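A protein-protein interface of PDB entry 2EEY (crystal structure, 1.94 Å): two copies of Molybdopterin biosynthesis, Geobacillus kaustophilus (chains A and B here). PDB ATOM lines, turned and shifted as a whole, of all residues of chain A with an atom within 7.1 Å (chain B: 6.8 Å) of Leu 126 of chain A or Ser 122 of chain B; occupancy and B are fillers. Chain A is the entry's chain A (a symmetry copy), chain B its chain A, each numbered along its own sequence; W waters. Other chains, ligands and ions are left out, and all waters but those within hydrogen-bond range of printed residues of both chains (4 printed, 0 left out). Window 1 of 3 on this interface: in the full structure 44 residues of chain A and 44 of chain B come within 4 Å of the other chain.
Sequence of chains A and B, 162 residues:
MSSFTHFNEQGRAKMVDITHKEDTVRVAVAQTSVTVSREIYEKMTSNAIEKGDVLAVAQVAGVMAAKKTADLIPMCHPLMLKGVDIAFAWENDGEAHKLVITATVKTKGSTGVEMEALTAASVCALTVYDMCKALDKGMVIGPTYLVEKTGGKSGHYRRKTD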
ATOM      1  N   THR A  32      38.211 -15.506   5.229  1.00  0.00           N
ATOM      2  CA  THR A  32      36.789 -15.793   5.248  1.00  0.00           C
ATOM      3  C   THR A  32      36.568 -16.958   4.298  1.00  0.00           C
ATOM      4  O   THR A  32      37.530 -17.571   3.818  1.00  0.00           O
ATOM      5  CB  THR A  32      35.927 -14.584   4.807  1.00  0.00           C
ATOM      6  OG1 THR A  32      34.547 -14.887   5.041  1.00  0.00           O
ATOM      7  CG2 THR A  32      36.120 -14.279   3.321  1.00  0.00           C
ATOM      8  N   VAL A  34      33.289 -19.144   1.651  1.00  0.00           N
ATOM      9  CA  VAL A  34      31.937 -19.243   1.140  1.00  0.00           C
ATOM     10  C   VAL A  34      31.656 -20.734   1.000  1.00  0.00           C
ATOM     11  O   VAL A  34      32.337 -21.430   0.248  1.00  0.00           O
ATOM     12  CB  VAL A  34      31.774 -18.570  -0.242  1.00  0.00           C
ATOM     13  CG1 VAL A  34      30.319 -18.656  -0.677  1.00  0.00           C
ATOM     14  CG2 VAL A  34      32.226 -17.111  -0.185  1.00  0.00           C
ATOM     15  N   ALA A  58      35.555 -11.851  -8.342  1.00  0.00           N
ATOM     16  CA  ALA A  58      35.569 -11.670  -6.896  1.00  0.00           C
ATOM     17  C   ALA A  58      36.898 -11.067  -6.441  1.00  0.00           C
ATOM     18  O   ALA A  58      36.935 -10.259  -5.513  1.00  0.00           O
ATOM     19  CB  ALA A  58      35.326 -13.010  -6.199  1.00  0.00           C
ATOM     20  N   ALA A  61      36.789  -7.357  -7.191  1.00  0.00           N
ATOM     21  CA  ALA A  61      35.904  -6.697  -6.232  1.00  0.00           C
ATOM     22  C   ALA A  61      36.588  -6.532  -4.877  1.00  0.00           C
ATOM     23  O   ALA A  61      36.484  -5.478  -4.241  1.00  0.00           O
ATOM     24  CB  ALA A  61      34.612  -7.499  -6.070  1.00  0.00           C
ATOM     25  N   ILE A  73      33.617   2.213   6.323  1.00  0.00           N
ATOM     26  CA  ILE A  73      33.778   2.131   7.775  1.00  0.00           C
ATOM     27  C   ILE A  73      33.936   3.559   8.286  1.00  0.00           C
ATOM     28  O   ILE A  73      34.981   4.177   8.104  1.00  0.00           O
ATOM     29  CB  ILE A  73      35.027   1.302   8.136  1.00  0.00           C
ATOM     30  CG1 ILE A  73      35.028  -0.004   7.332  1.00  0.00           C
ATOM     31  CG2 ILE A  73      35.057   1.024   9.637  1.00  0.00           C
ATOM     32  CD1 ILE A  73      33.745  -0.830   7.460  1.00  0.00           C
ATOM     33  N   ILE A 101      38.979 -17.805   1.380  1.00  0.00           N
ATOM     34  CA  ILE A 101      39.492 -16.559   0.825  1.00  0.00           C
ATOM     35  C   ILE A 101      40.447 -15.891   1.809  1.00  0.00           C
ATOM     36  O   ILE A 101      40.094 -15.683   2.969  1.00  0.00           O
ATOM     37  CB  ILE A 101      38.316 -15.592   0.535  1.00  0.00           C
ATOM     38  CG1 ILE A 101      37.343 -16.246  -0.446  1.00  0.00           C
ATOM     39  CG2 ILE A 101      38.839 -14.270   0.016  1.00  0.00           C
ATOM     40  CD1 ILE A 101      35.967 -15.581  -0.499  1.00  0.00           C
ATOM     41  N   THR A 119      37.687  -6.047   5.113  1.00  0.00           N
ATOM     42  CA  THR A 119      36.700  -5.556   4.164  1.00  0.00           C
ATOM     43  C   THR A 119      36.931  -6.177   2.786  1.00  0.00           C
ATOM     44  O   THR A 119      35.980  -6.534   2.095  1.00  0.00           O
ATOM     45  CB  THR A 119      36.753  -4.023   4.060  1.00  0.00           C
ATOM     46  OG1 THR A 119      36.409  -3.452   5.333  1.00  0.00           O
ATOM     47  CG2 THR A 119      35.773  -3.523   3.009  1.00  0.00           C
ATOM     48  N   ALA A 120      38.197  -6.301   2.399  1.00  0.00           N
ATOM     49  CA  ALA A 120      38.549  -6.892   1.111  1.00  0.00           C
ATOM     50  C   ALA A 120      38.017  -8.319   1.077  1.00  0.00           C
ATOM     51  O   ALA A 120      37.389  -8.735   0.104  1.00  0.00           O
ATOM     52  CB  ALA A 120      40.074  -6.891   0.925  1.00  0.00           C
ATOM     53  N   ALA A 121      38.271  -9.068   2.147  1.00  0.00           N
ATOM     54  CA  ALA A 121      37.807 -10.450   2.227  1.00  0.00           C
ATOM     55  C   ALA A 121      36.278 -10.541   2.199  1.00  0.00           C
ATOM     56  O   ALA A 121      35.720 -11.381   1.498  1.00  0.00           O
ATOM     57  CB  ALA A 121      38.345 -11.112   3.499  1.00  0.00           C
ATOM     58  N   SER A 122      35.608  -9.677   2.960  1.00  0.00           N
ATOM     59  CA  SER A 122      34.144  -9.676   3.023  1.00  0.00           C
ATOM     60  C   SER A 122      33.479  -9.414   1.676  1.00  0.00           C
ATOM     61  O   SER A 122      32.536 -10.110   1.299  1.00  0.00           O
ATOM     62  CB  SER A 122      33.646  -8.626   4.023  1.00  0.00           C
ATOM     63  OG  SER A 122      34.094  -8.902   5.337  1.00  0.00           O
ATOM     64  N   VAL A 123      33.958  -8.400   0.958  1.00  0.00           N
ATOM     65  CA  VAL A 123      33.371  -8.064  -0.337  1.00  0.00           C
ATOM     66  C   VAL A 123      33.728  -9.112  -1.390  1.00  0.00           C
ATOM     67  O   VAL A 123      32.946  -9.375  -2.302  1.00  0.00           O
ATOM     68  CB  VAL A 123      33.807  -6.656  -0.799  1.00  0.00           C
ATOM     69  CG1 VAL A 123      33.296  -6.380  -2.217  1.00  0.00           C
ATOM     70  CG2 VAL A 123      33.240  -5.606   0.163  1.00  0.00           C
ATOM     71  N   CYS A 124      34.909  -9.709  -1.260  1.00  0.00           N
ATOM     72  CA  CYS A 124      35.316 -10.757  -2.184  1.00  0.00           C
ATOM     73  C   CYS A 124      34.288 -11.891  -2.044  1.00  0.00           C
ATOM     74  O   CYS A 124      33.772 -12.406  -3.038  1.00  0.00           O
ATOM     75  CB  CYS A 124      36.720 -11.263  -1.825  1.00  0.00           C
ATOM     76  SG  CYS A 124      37.331 -12.605  -2.879  1.00  0.00           S
ATOM     77  N   ALA A 125      33.980 -12.260  -0.801  1.00  0.00           N
ATOM     78  CA  ALA A 125      33.010 -13.322  -0.534  1.00  0.00           C
ATOM     79  C   ALA A 125      31.625 -12.941  -1.060  1.00  0.00           C
ATOM     80  O   ALA A 125      30.957 -13.746  -1.707  1.00  0.00           O
ATOM     81  CB  ALA A 125      32.944 -13.613   0.975  1.00  0.00           C
ATOM     82  N   LEU A 126      31.193 -11.713  -0.787  1.00  0.00           N
ATOM     83  CA  LEU A 126      29.886 -11.256  -1.256  1.00  0.00           C
ATOM     84  C   LEU A 126      29.792 -11.325  -2.778  1.00  0.00           C
ATOM     85  O   LEU A 126      28.725 -11.584  -3.325  1.00  0.00           O
ATOM     86  CB  LEU A 126      29.624  -9.819  -0.790  1.00  0.00           C
ATOM     87  CG  LEU A 126      29.324  -9.642   0.706  1.00  0.00           C
ATOM     88  CD1 LEU A 126      29.479  -8.182   1.113  1.00  0.00           C
ATOM     89  CD2 LEU A 126      27.901 -10.127   0.992  1.00  0.00           C
ATOM     90  N   THR A 127      30.909 -11.096  -3.461  1.00  0.00           N
ATOM     91  CA  THR A 127      30.908 -11.130  -4.917  1.00  0.00           C
ATOM     92  C   THR A 127      30.792 -12.564  -5.431  1.00  0.00           C
ATOM     93  O   THR A 127      30.141 -12.814  -6.442  1.00  0.00           O
ATOM     94  CB  THR A 127      32.159 -10.432  -5.481  1.00  0.00           C
ATOM     95  OG1 THR A 127      32.128  -9.051  -5.087  1.00  0.00           O
ATOM     96  CG2 THR A 127      32.176 -10.500  -7.014  1.00  0.00           C
ATOM     97  N   VAL A 128      31.417 -13.507  -4.733  1.00  0.00           N
ATOM     98  CA  VAL A 128      31.300 -14.912  -5.124  1.00  0.00           C
ATOM     99  C   VAL A 128      29.813 -15.254  -4.994  1.00  0.00           C
ATOM    100  O   VAL A 128      29.224 -15.884  -5.879  1.00  0.00           O
ATOM    101  CB  VAL A 128      32.113 -15.834  -4.189  1.00  0.00           C
ATOM    102  CG1 VAL A 128      31.779 -17.298  -4.476  1.00  0.00           C
ATOM    103  CG2 VAL A 128      33.607 -15.583  -4.381  1.00  0.00           C
ATOM    104  N   TYR A 129      29.210 -14.819  -3.887  1.00  0.00           N
ATOM    105  CA  TYR A 129      27.789 -15.065  -3.639  1.00  0.00           C
ATOM    106  C   TYR A 129      26.934 -14.456  -4.754  1.00  0.00           C
ATOM    107  O   TYR A 129      26.030 -15.109  -5.279  1.00  0.00           O
ATOM    108  CB  TYR A 129      27.377 -14.483  -2.272  1.00  0.00           C
ATOM    109  CG  TYR A 129      25.937 -14.761  -1.878  1.00  0.00           C
ATOM    110  CD1 TYR A 129      24.880 -14.140  -2.544  1.00  0.00           C
ATOM    111  CD2 TYR A 129      25.629 -15.674  -0.866  1.00  0.00           C
ATOM    112  CE1 TYR A 129      23.556 -14.423  -2.222  1.00  0.00           C
ATOM    113  CE2 TYR A 129      24.295 -15.966  -0.534  1.00  0.00           C
ATOM    114  CZ  TYR A 129      23.271 -15.335  -1.221  1.00  0.00           C
ATOM    115  OH  TYR A 129      21.954 -15.623  -0.931  1.00  0.00           O
ATOM    116  N   ASP A 130      27.220 -13.212  -5.127  1.00  0.00           N
ATOM    117  CA  ASP A 130      26.445 -12.564  -6.183  1.00  0.00           C
ATOM    118  C   ASP A 130      26.531 -13.319  -7.514  1.00  0.00           C
ATOM    119  O   ASP A 130      25.532 -13.477  -8.219  1.00  0.00           O
ATOM    120  CB  ASP A 130      26.928 -11.130  -6.403  1.00  0.00           C
ATOM    121  CG  ASP A 130      26.147 -10.420  -7.493  1.00  0.00           C
ATOM    122  OD1 ASP A 130      24.915 -10.293  -7.340  1.00  0.00           O
ATOM    123  OD2 ASP A 130      26.758  -9.994  -8.500  1.00  0.00           O
ATOM    124  N   MET A 131      27.727 -13.789  -7.845  1.00  0.00           N
ATOM    125  CA  MET A 131      27.943 -14.496  -9.106  1.00  0.00           C
ATOM    126  C   MET A 131      27.334 -15.895  -9.166  1.00  0.00           C
ATOM    127  O   MET A 131      27.084 -16.420 -10.255  1.00  0.00           O
ATOM    128  CB  MET A 131      29.448 -14.587  -9.406  1.00  0.00           C
ATOM    129  CG  MET A 131      30.155 -13.244  -9.621  1.00  0.00           C
ATOM    130  SD  MET A 131      29.500 -12.239 -10.997  1.00  0.00           S
ATOM    131  CE  MET A 131      30.202 -13.111 -12.430  1.00  0.00           C
ATOM    132  N   CYS A 132      27.090 -16.502  -8.007  1.00  0.00           N
ATOM    133  CA  CYS A 132      26.535 -17.854  -7.973  1.00  0.00           C
ATOM    134  C   CYS A 132      25.115 -17.976  -7.426  1.00  0.00           C
ATOM    135  O   CYS A 132      24.523 -19.057  -7.487  1.00  0.00           O
ATOM    136  CB  CYS A 132      27.444 -18.769  -7.144  1.00  0.00           C
ATOM    137  SG  CYS A 132      29.168 -18.786  -7.662  1.00  0.00           S
ATOM    138  N   ILE A 141      28.457 -17.346   4.061  1.00  0.00           N
ATOM    139  CA  ILE A 141      29.722 -16.622   4.083  1.00  0.00           C
ATOM    140  C   ILE A 141      30.315 -16.600   5.485  1.00  0.00           C
ATOM    141  O   ILE A 141      29.604 -16.375   6.465  1.00  0.00           O
ATOM    142  CB  ILE A 141      29.533 -15.151   3.611  1.00  0.00           C
ATOM    143  CG1 ILE A 141      29.096 -15.122   2.144  1.00  0.00           C
ATOM    144  CG2 ILE A 141      30.832 -14.359   3.800  1.00  0.00           C
ATOM    145  CD1 ILE A 141      28.765 -13.727   1.630  1.00  0.00           C
ATOM    146  N   THR B  32      23.940 -11.912  10.246  1.00  0.00           N
ATOM    147  CA  THR B  32      25.336 -12.174  10.544  1.00  0.00           C
ATOM    148  C   THR B  32      25.511 -11.944  12.036  1.00  0.00           C
ATOM    149  O   THR B  32      24.528 -11.763  12.765  1.00  0.00           O
ATOM    150  CB  THR B  32      26.300 -11.255   9.753  1.00  0.00           C
ATOM    151  OG1 THR B  32      27.643 -11.708   9.957  1.00  0.00           O
ATOM    152  CG2 THR B  32      26.192  -9.804  10.222  1.00  0.00           C
ATOM    153  N   ALA B  65      25.888   1.297   3.649  1.00  0.00           N
ATOM    154  CA  ALA B  65      26.482   0.236   2.836  1.00  0.00           C
ATOM    155  C   ALA B  65      25.441  -0.362   1.881  1.00  0.00           C
ATOM    156  O   ALA B  65      25.761  -0.730   0.750  1.00  0.00           O
ATOM    157  CB  ALA B  65      27.059  -0.856   3.733  1.00  0.00           C
ATOM    158  N   LEU B  72      30.140  -1.609  -4.896  1.00  0.00           N
ATOM    159  CA  LEU B  72      31.049  -2.651  -4.406  1.00  0.00           C
ATOM    160  C   LEU B  72      30.963  -4.003  -5.101  1.00  0.00           C
ATOM    161  O   LEU B  72      31.981  -4.671  -5.288  1.00  0.00           O
ATOM    162  CB  LEU B  72      30.812  -2.866  -2.912  1.00  0.00           C
ATOM    163  CG  LEU B  72      30.961  -1.661  -1.986  1.00  0.00           C
ATOM    164  CD1 LEU B  72      30.402  -2.018  -0.616  1.00  0.00           C
ATOM    165  CD2 LEU B  72      32.430  -1.247  -1.896  1.00  0.00           C
ATOM    166  N   ILE B  73      29.750  -4.417  -5.450  1.00  0.00           N
ATOM    167  CA  ILE B  73      29.523  -5.704  -6.109  1.00  0.00           C
ATOM    168  C   ILE B  73      29.447  -5.428  -7.607  1.00  0.00           C
ATOM    169  O   ILE B  73      28.458  -4.888  -8.095  1.00  0.00           O
ATOM    170  CB  ILE B  73      28.203  -6.337  -5.623  1.00  0.00           C
ATOM    171  CG1 ILE B  73      28.142  -6.287  -4.092  1.00  0.00           C
ATOM    172  CG2 ILE B  73      28.091  -7.772  -6.132  1.00  0.00           C
ATOM    173  CD1 ILE B  73      29.355  -6.900  -3.387  1.00  0.00           C
ATOM    174  N   ILE B 101      23.170  -9.663  14.123  1.00  0.00           N
ATOM    175  CA  ILE B 101      22.771  -8.528  13.300  1.00  0.00           C
ATOM    176  C   ILE B 101      21.827  -8.981  12.191  1.00  0.00           C
ATOM    177  O   ILE B 101      22.144  -9.908  11.447  1.00  0.00           O
ATOM    178  CB  ILE B 101      24.025  -7.884  12.657  1.00  0.00           C
ATOM    179  CG1 ILE B 101      24.989  -7.428  13.753  1.00  0.00           C
ATOM    180  CG2 ILE B 101      23.621  -6.742  11.749  1.00  0.00           C
ATOM    181  CD1 ILE B 101      26.410  -7.152  13.260  1.00  0.00           C
ATOM    182  N   ALA B 103      19.649  -7.526   8.915  1.00  0.00           N
ATOM    183  CA  ALA B 103      19.366  -6.413   8.017  1.00  0.00           C
ATOM    184  C   ALA B 103      18.221  -6.712   7.062  1.00  0.00           C
ATOM    185  O   ALA B 103      18.202  -7.757   6.407  1.00  0.00           O
ATOM    186  CB  ALA B 103      20.626  -6.049   7.226  1.00  0.00           C
ATOM    187  N   GLU B 114      18.831  -9.140  -2.311  1.00  0.00           N
ATOM    188  CA  GLU B 114      19.580 -10.037  -1.437  1.00  0.00           C
ATOM    189  C   GLU B 114      20.981  -9.483  -1.177  1.00  0.00           C
ATOM    190  O   GLU B 114      21.465  -9.506  -0.047  1.00  0.00           O
ATOM    191  CB  GLU B 114      19.701 -11.434  -2.061  1.00  0.00           C
ATOM    192  CG  GLU B 114      18.379 -12.050  -2.460  1.00  0.00           C
ATOM    193  CD  GLU B 114      18.072 -11.853  -3.931  1.00  0.00           C
ATOM    194  OE1 GLU B 114      18.357 -10.758  -4.459  1.00  0.00           O
ATOM    195  OE2 GLU B 114      17.538 -12.794  -4.555  1.00  0.00           O
ATOM    196  N   MET B 115      21.632  -8.978  -2.221  1.00  0.00           N
ATOM    197  CA  MET B 115      22.985  -8.445  -2.064  1.00  0.00           C
ATOM    198  C   MET B 115      23.027  -7.200  -1.177  1.00  0.00           C
ATOM    199  O   MET B 115      23.979  -6.999  -0.418  1.00  0.00           O
ATOM    200  CB  MET B 115      23.596  -8.127  -3.428  1.00  0.00           C
ATOM    201  CG  MET B 115      23.821  -9.357  -4.310  1.00  0.00           C
ATOM    202  SD  MET B 115      24.580 -10.746  -3.424  1.00  0.00           S
ATOM    203  CE  MET B 115      25.996  -9.951  -2.620  1.00  0.00           C
ATOM    204  N   ALA B 117      21.001  -6.523   1.303  1.00  0.00           N
ATOM    205  CA  ALA B 117      20.810  -6.967   2.683  1.00  0.00           C
ATOM    206  C   ALA B 117      22.082  -7.615   3.225  1.00  0.00           C
ATOM    207  O   ALA B 117      22.495  -7.345   4.355  1.00  0.00           O
ATOM    208  CB  ALA B 117      19.643  -7.951   2.765  1.00  0.00           C
ATOM    209  N   LEU B 118      22.699  -8.471   2.415  1.00  0.00           N
ATOM    210  CA  LEU B 118      23.931  -9.155   2.811  1.00  0.00           C
ATOM    211  C   LEU B 118      25.080  -8.170   3.003  1.00  0.00           C
ATOM    212  O   LEU B 118      25.893  -8.317   3.915  1.00  0.00           O
ATOM    213  CB  LEU B 118      24.320 -10.195   1.752  1.00  0.00           C
ATOM    214  CG  LEU B 118      23.420 -11.438   1.688  1.00  0.00           C
ATOM    215  CD1 LEU B 118      23.644 -12.181   0.374  1.00  0.00           C
ATOM    216  CD2 LEU B 118      23.714 -12.332   2.879  1.00  0.00           C
ATOM    217  N   THR B 119      25.149  -7.166   2.136  1.00  0.00           N
ATOM    218  CA  THR B 119      26.208  -6.173   2.225  1.00  0.00           C
ATOM    219  C   THR B 119      25.991  -5.270   3.440  1.00  0.00           C
ATOM    220  O   THR B 119      26.941  -4.918   4.133  1.00  0.00           O
ATOM    221  CB  THR B 119      26.269  -5.320   0.947  1.00  0.00           C
ATOM    222  OG1 THR B 119      26.600  -6.164  -0.167  1.00  0.00           O
ATOM    223  CG2 THR B 119      27.326  -4.233   1.080  1.00  0.00           C
ATOM    224  N   ALA B 120      24.736  -4.905   3.687  1.00  0.00           N
ATOM    225  CA  ALA B 120      24.396  -4.057   4.826  1.00  0.00           C
ATOM    226  C   ALA B 120      24.825  -4.773   6.102  1.00  0.00           C
ATOM    227  O   ALA B 120      25.461  -4.181   6.973  1.00  0.00           O
ATOM    228  CB  ALA B 120      22.884  -3.786   4.855  1.00  0.00           C
ATOM    229  N   ALA B 121      24.473  -6.052   6.206  1.00  0.00           N
ATOM    230  CA  ALA B 121      24.833  -6.839   7.382  1.00  0.00           C
ATOM    231  C   ALA B 121      26.351  -6.970   7.539  1.00  0.00           C
ATOM    232  O   ALA B 121      26.876  -6.820   8.639  1.00  0.00           O
ATOM    233  CB  ALA B 121      24.196  -8.230   7.299  1.00  0.00           C
ATOM    234  N   SER B 122      27.049  -7.249   6.439  1.00  0.00           N
ATOM    235  CA  SER B 122      28.505  -7.410   6.468  1.00  0.00           C
ATOM    236  C   SER B 122      29.243  -6.161   6.941  1.00  0.00           C
ATOM    237  O   SER B 122      30.148  -6.247   7.771  1.00  0.00           O
ATOM    238  CB  SER B 122      29.036  -7.791   5.081  1.00  0.00           C
ATOM    239  OG  SER B 122      28.514  -9.033   4.646  1.00  0.00           O
ATOM    240  N   VAL B 123      28.869  -5.003   6.401  1.00  0.00           N
ATOM    241  CA  VAL B 123      29.533  -3.758   6.780  1.00  0.00           C
ATOM    242  C   VAL B 123      29.145  -3.339   8.197  1.00  0.00           C
ATOM    243  O   VAL B 123      29.943  -2.736   8.913  1.00  0.00           O
ATOM    244  CB  VAL B 123      29.218  -2.629   5.773  1.00  0.00           C
ATOM    245  CG1 VAL B 123      29.806  -1.301   6.263  1.00  0.00           C
ATOM    246  CG2 VAL B 123      29.819  -2.983   4.408  1.00  0.00           C
ATOM    247  N   CYS B 124      27.919  -3.662   8.600  1.00  0.00           N
ATOM    248  CA  CYS B 124      27.477  -3.352   9.951  1.00  0.00           C
ATOM    249  C   CYS B 124      28.413  -4.108  10.906  1.00  0.00           C
ATOM    250  O   CYS B 124      28.932  -3.540  11.869  1.00  0.00           O
ATOM    251  CB  CYS B 124      26.027  -3.812  10.151  1.00  0.00           C
ATOM    252  SG  CYS B 124      25.365  -3.520  11.814  1.00  0.00           S
ATOM    253  N   ALA B 125      28.642  -5.390  10.619  1.00  0.00           N
ATOM    254  CA  ALA B 125      29.521  -6.216  11.446  1.00  0.00           C
ATOM    255  C   ALA B 125      30.950  -5.672  11.436  1.00  0.00           C
ATOM    256  O   ALA B 125      31.586  -5.559  12.483  1.00  0.00           O
ATOM    257  CB  ALA B 125      29.502  -7.672  10.947  1.00  0.00           C
ATOM    258  N   LEU B 126      31.458  -5.332  10.255  1.00  0.00           N
ATOM    259  CA  LEU B 126      32.813  -4.793  10.147  1.00  0.00           C
ATOM    260  C   LEU B 126      32.965  -3.517  10.970  1.00  0.00           C
ATOM    261  O   LEU B 126      34.033  -3.249  11.511  1.00  0.00           O
ATOM    262  CB  LEU B 126      33.159  -4.505   8.682  1.00  0.00           C
ATOM    263  CG  LEU B 126      33.408  -5.734   7.795  1.00  0.00           C
ATOM    264  CD1 LEU B 126      33.342  -5.353   6.322  1.00  0.00           C
ATOM    265  CD2 LEU B 126      34.778  -6.324   8.132  1.00  0.00           C
ATOM    266  N   THR B 127      31.897  -2.731  11.066  1.00  0.00           N
ATOM    267  CA  THR B 127      31.956  -1.488  11.821  1.00  0.00           C
ATOM    268  C   THR B 127      31.990  -1.762  13.324  1.00  0.00           C
ATOM    269  O   THR B 127      32.663  -1.056  14.072  1.00  0.00           O
ATOM    270  CB  THR B 127      30.784  -0.564  11.445  1.00  0.00           C
ATOM    271  OG1 THR B 127      30.898  -0.224  10.055  1.00  0.00           O
ATOM    272  CG2 THR B 127      30.826   0.731  12.268  1.00  0.00           C
ATOM    273  N   ILE B 141      33.576 -12.516  12.829  1.00  0.00           N
ATOM    274  CA  ILE B 141      32.367 -12.085  12.138  1.00  0.00           C
ATOM    275  C   ILE B 141      31.719 -13.245  11.395  1.00  0.00           C
ATOM    276  O   ILE B 141      32.402 -14.033  10.741  1.00  0.00           O
ATOM    277  CB  ILE B 141      32.681 -10.962  11.107  1.00  0.00           C
ATOM    278  CG1 ILE B 141      33.180  -9.709  11.832  1.00  0.00           C
ATOM    279  CG2 ILE B 141      31.435 -10.639  10.274  1.00  0.00           C
ATOM    280  CD1 ILE B 141      33.632  -8.597  10.895  1.00  0.00           C
ATOM    281  N   THR B 144      27.539 -15.347   7.756  1.00  0.00           N
ATOM    282  CA  THR B 144      26.630 -14.377   7.155  1.00  0.00           C
ATOM    283  C   THR B 144      25.812 -15.124   6.108  1.00  0.00           C
ATOM    284  O   THR B 144      26.367 -15.835   5.267  1.00  0.00           O
ATOM    285  CB  THR B 144      27.431 -13.240   6.482  1.00  0.00           C
ATOM    286  OG1 THR B 144      28.258 -12.604   7.465  1.00  0.00           O
ATOM    287  CG2 THR B 144      26.500 -12.211   5.855  1.00  0.00           C
HETATM  288  O   HOH W   1      31.761  -8.756   6.985  1.00  0.00           O
HETATM  289  O   HOH W   2      30.780 -10.556   3.795  1.00  0.00           O
HETATM  290  O   HOH W   3      34.392  -3.622  -4.645  1.00  0.00           O
HETATM  291  O   HOH W   4      31.078 -13.654   7.705  1.00  0.00           O
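The side-chain hydroxyl (OG) of Ser 122 of chain B sits at hydrogen-bond distance from the backbone carbonyl oxygen (O) of Leu 118 of chain B, at 2.8 Å.
O of Val 123 of chain A lies within hydrogen-bond range of OG1 of Thr 127 of chain A.
OG1 of Thr 127 of chain B lies within hydrogen-bond range of O of Val 123 of chain B, at 2.9 Å.
O of Met 115 of chain B lies within hydrogen-bond range of OG1 of Thr 119 of chain B, 2.8 Å away.
The side-chain hydroxyl (OG1) of Thr 32 of chain B lies within hydrogen-bond range of the side-chain hydroxyl (OG1) of Thr 144 of chain B.
Of the 21 printed residues of chain A, 10 touch a printed residue of chain B.
Printed residues of chain A that touch a printed residue of chain B: Ala 61, Ile 73, Thr 119, Ser 122, Val 123, Leu 126, Thr 127, Tyr 129, Asp 130 and Ile 141.
Among the printed residues, 17 pairs touch across the chains.
Among the printed residues, no Asp or Glu carboxylate lies within 4 Å of a Lys or Arg side-chain nitrogen of the other chain.
Of chain B, only Ile 73, Met 115, Leu 118, Thr 119 and Ser 122 come within 4 Å of Leu 126 of chain A.
Of the printed residues of chain B, Asp 130 of chain A touches Ile 73 and Met 115.
Printed residues of chain A within 4 Å of Leu 72 of chain B: Ala 61 (3.9 Å) and Val 123 (3.8 Å).
Ser 122 of chain B touches one residue of chain A.
Printed residues of chain A within 4 Å of Leu 126 of chain B: Ile 73, Thr 119 and Ser 122.
Of the printed residues of chain A, Thr 144 of chain B touches Ile 141.
Ile 73 of chain A touches Leu 126 of chain B, and with the chains exchanged Leu 126 of chain A touches Ile 73 of chain B.
Ile 73 of chain A touches Thr 127 of chain B, and with the chains exchanged Thr 127 of chain A touches Ile 73 of chain B.
Thr 119 of chain A touches Leu 126 of chain B, and with the chains exchanged Leu 126 of chain A touches Thr 119 of chain B.
Ser 122 of chain A touches Leu 126 of chain B, and with the chains exchanged Leu 126 of chain A touches Ser 122 of chain B.
Positions printed for both chains: 32, 73, 101, 119, 120, 121, 122, 123, 124, 125, 126, 127 and 141.
Of the 17 pairs that touch across the chains among the printed residues, 8 have their exchanged pair printed and touching as well.
Water W3 lies within hydrogen-bond range of O of Leu 72 of chain B (2.7 Å) and O of Ala 61 of chain A (2.8 Å).
Water W2 bridges the side-chain hydroxyl of Ser 122 of chain B (2.9 Å) and the backbone carbonyl oxygen of Ser 122 of chain A (3.1 Å).
Water W1 lies within hydrogen-bond range of the side-chain hydroxyl of Ser 122 of chain A and the backbone carbonyl oxygen of Ser 122 of chain B.
Water W4 lies within hydrogen-bond range of OG1 of Thr 144 of chain B (3.0 Å), O of Ile 141 of chain A (3.3 Å) and O of Ile 141 of chain B (3.3 Å).
CB of Ala 61 of chain A touches O of Leu 72 of chain B, at 3.9 Å.
CD1 of Ile 73 of chain A touches CB of Leu 126 of chain B, at 3.9 Å.
CD1 of Leu 126 of chain B touches OG1 of Thr 119 of chain A (3.7 Å).
Ser 122 of chain A touches Leu 126 of chain B.
CG1 of Val 123 of chain A touches O of Leu 72 of chain B, at 3.8 Å.
CD1 of Leu 126 of chain A touches OG1 of Thr 119 of chain B (3.7 Å).
CD1 of Ile 73 of chain B touches OG1 of Thr 127 of chain A, 3.9 Å away.
Tyr 129 of chain A touches Met 115 of chain B.
Ile 73 of chain B touches Asp 130 of chain A.
Asp 130 of chain A touches Met 115 of chain B (OD1 to CG, 3.4 Å).
O of Ile 141 of chain A sits at hydrogen-bond distance from N of Thr 144 of chain B, 2.6 Å away.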
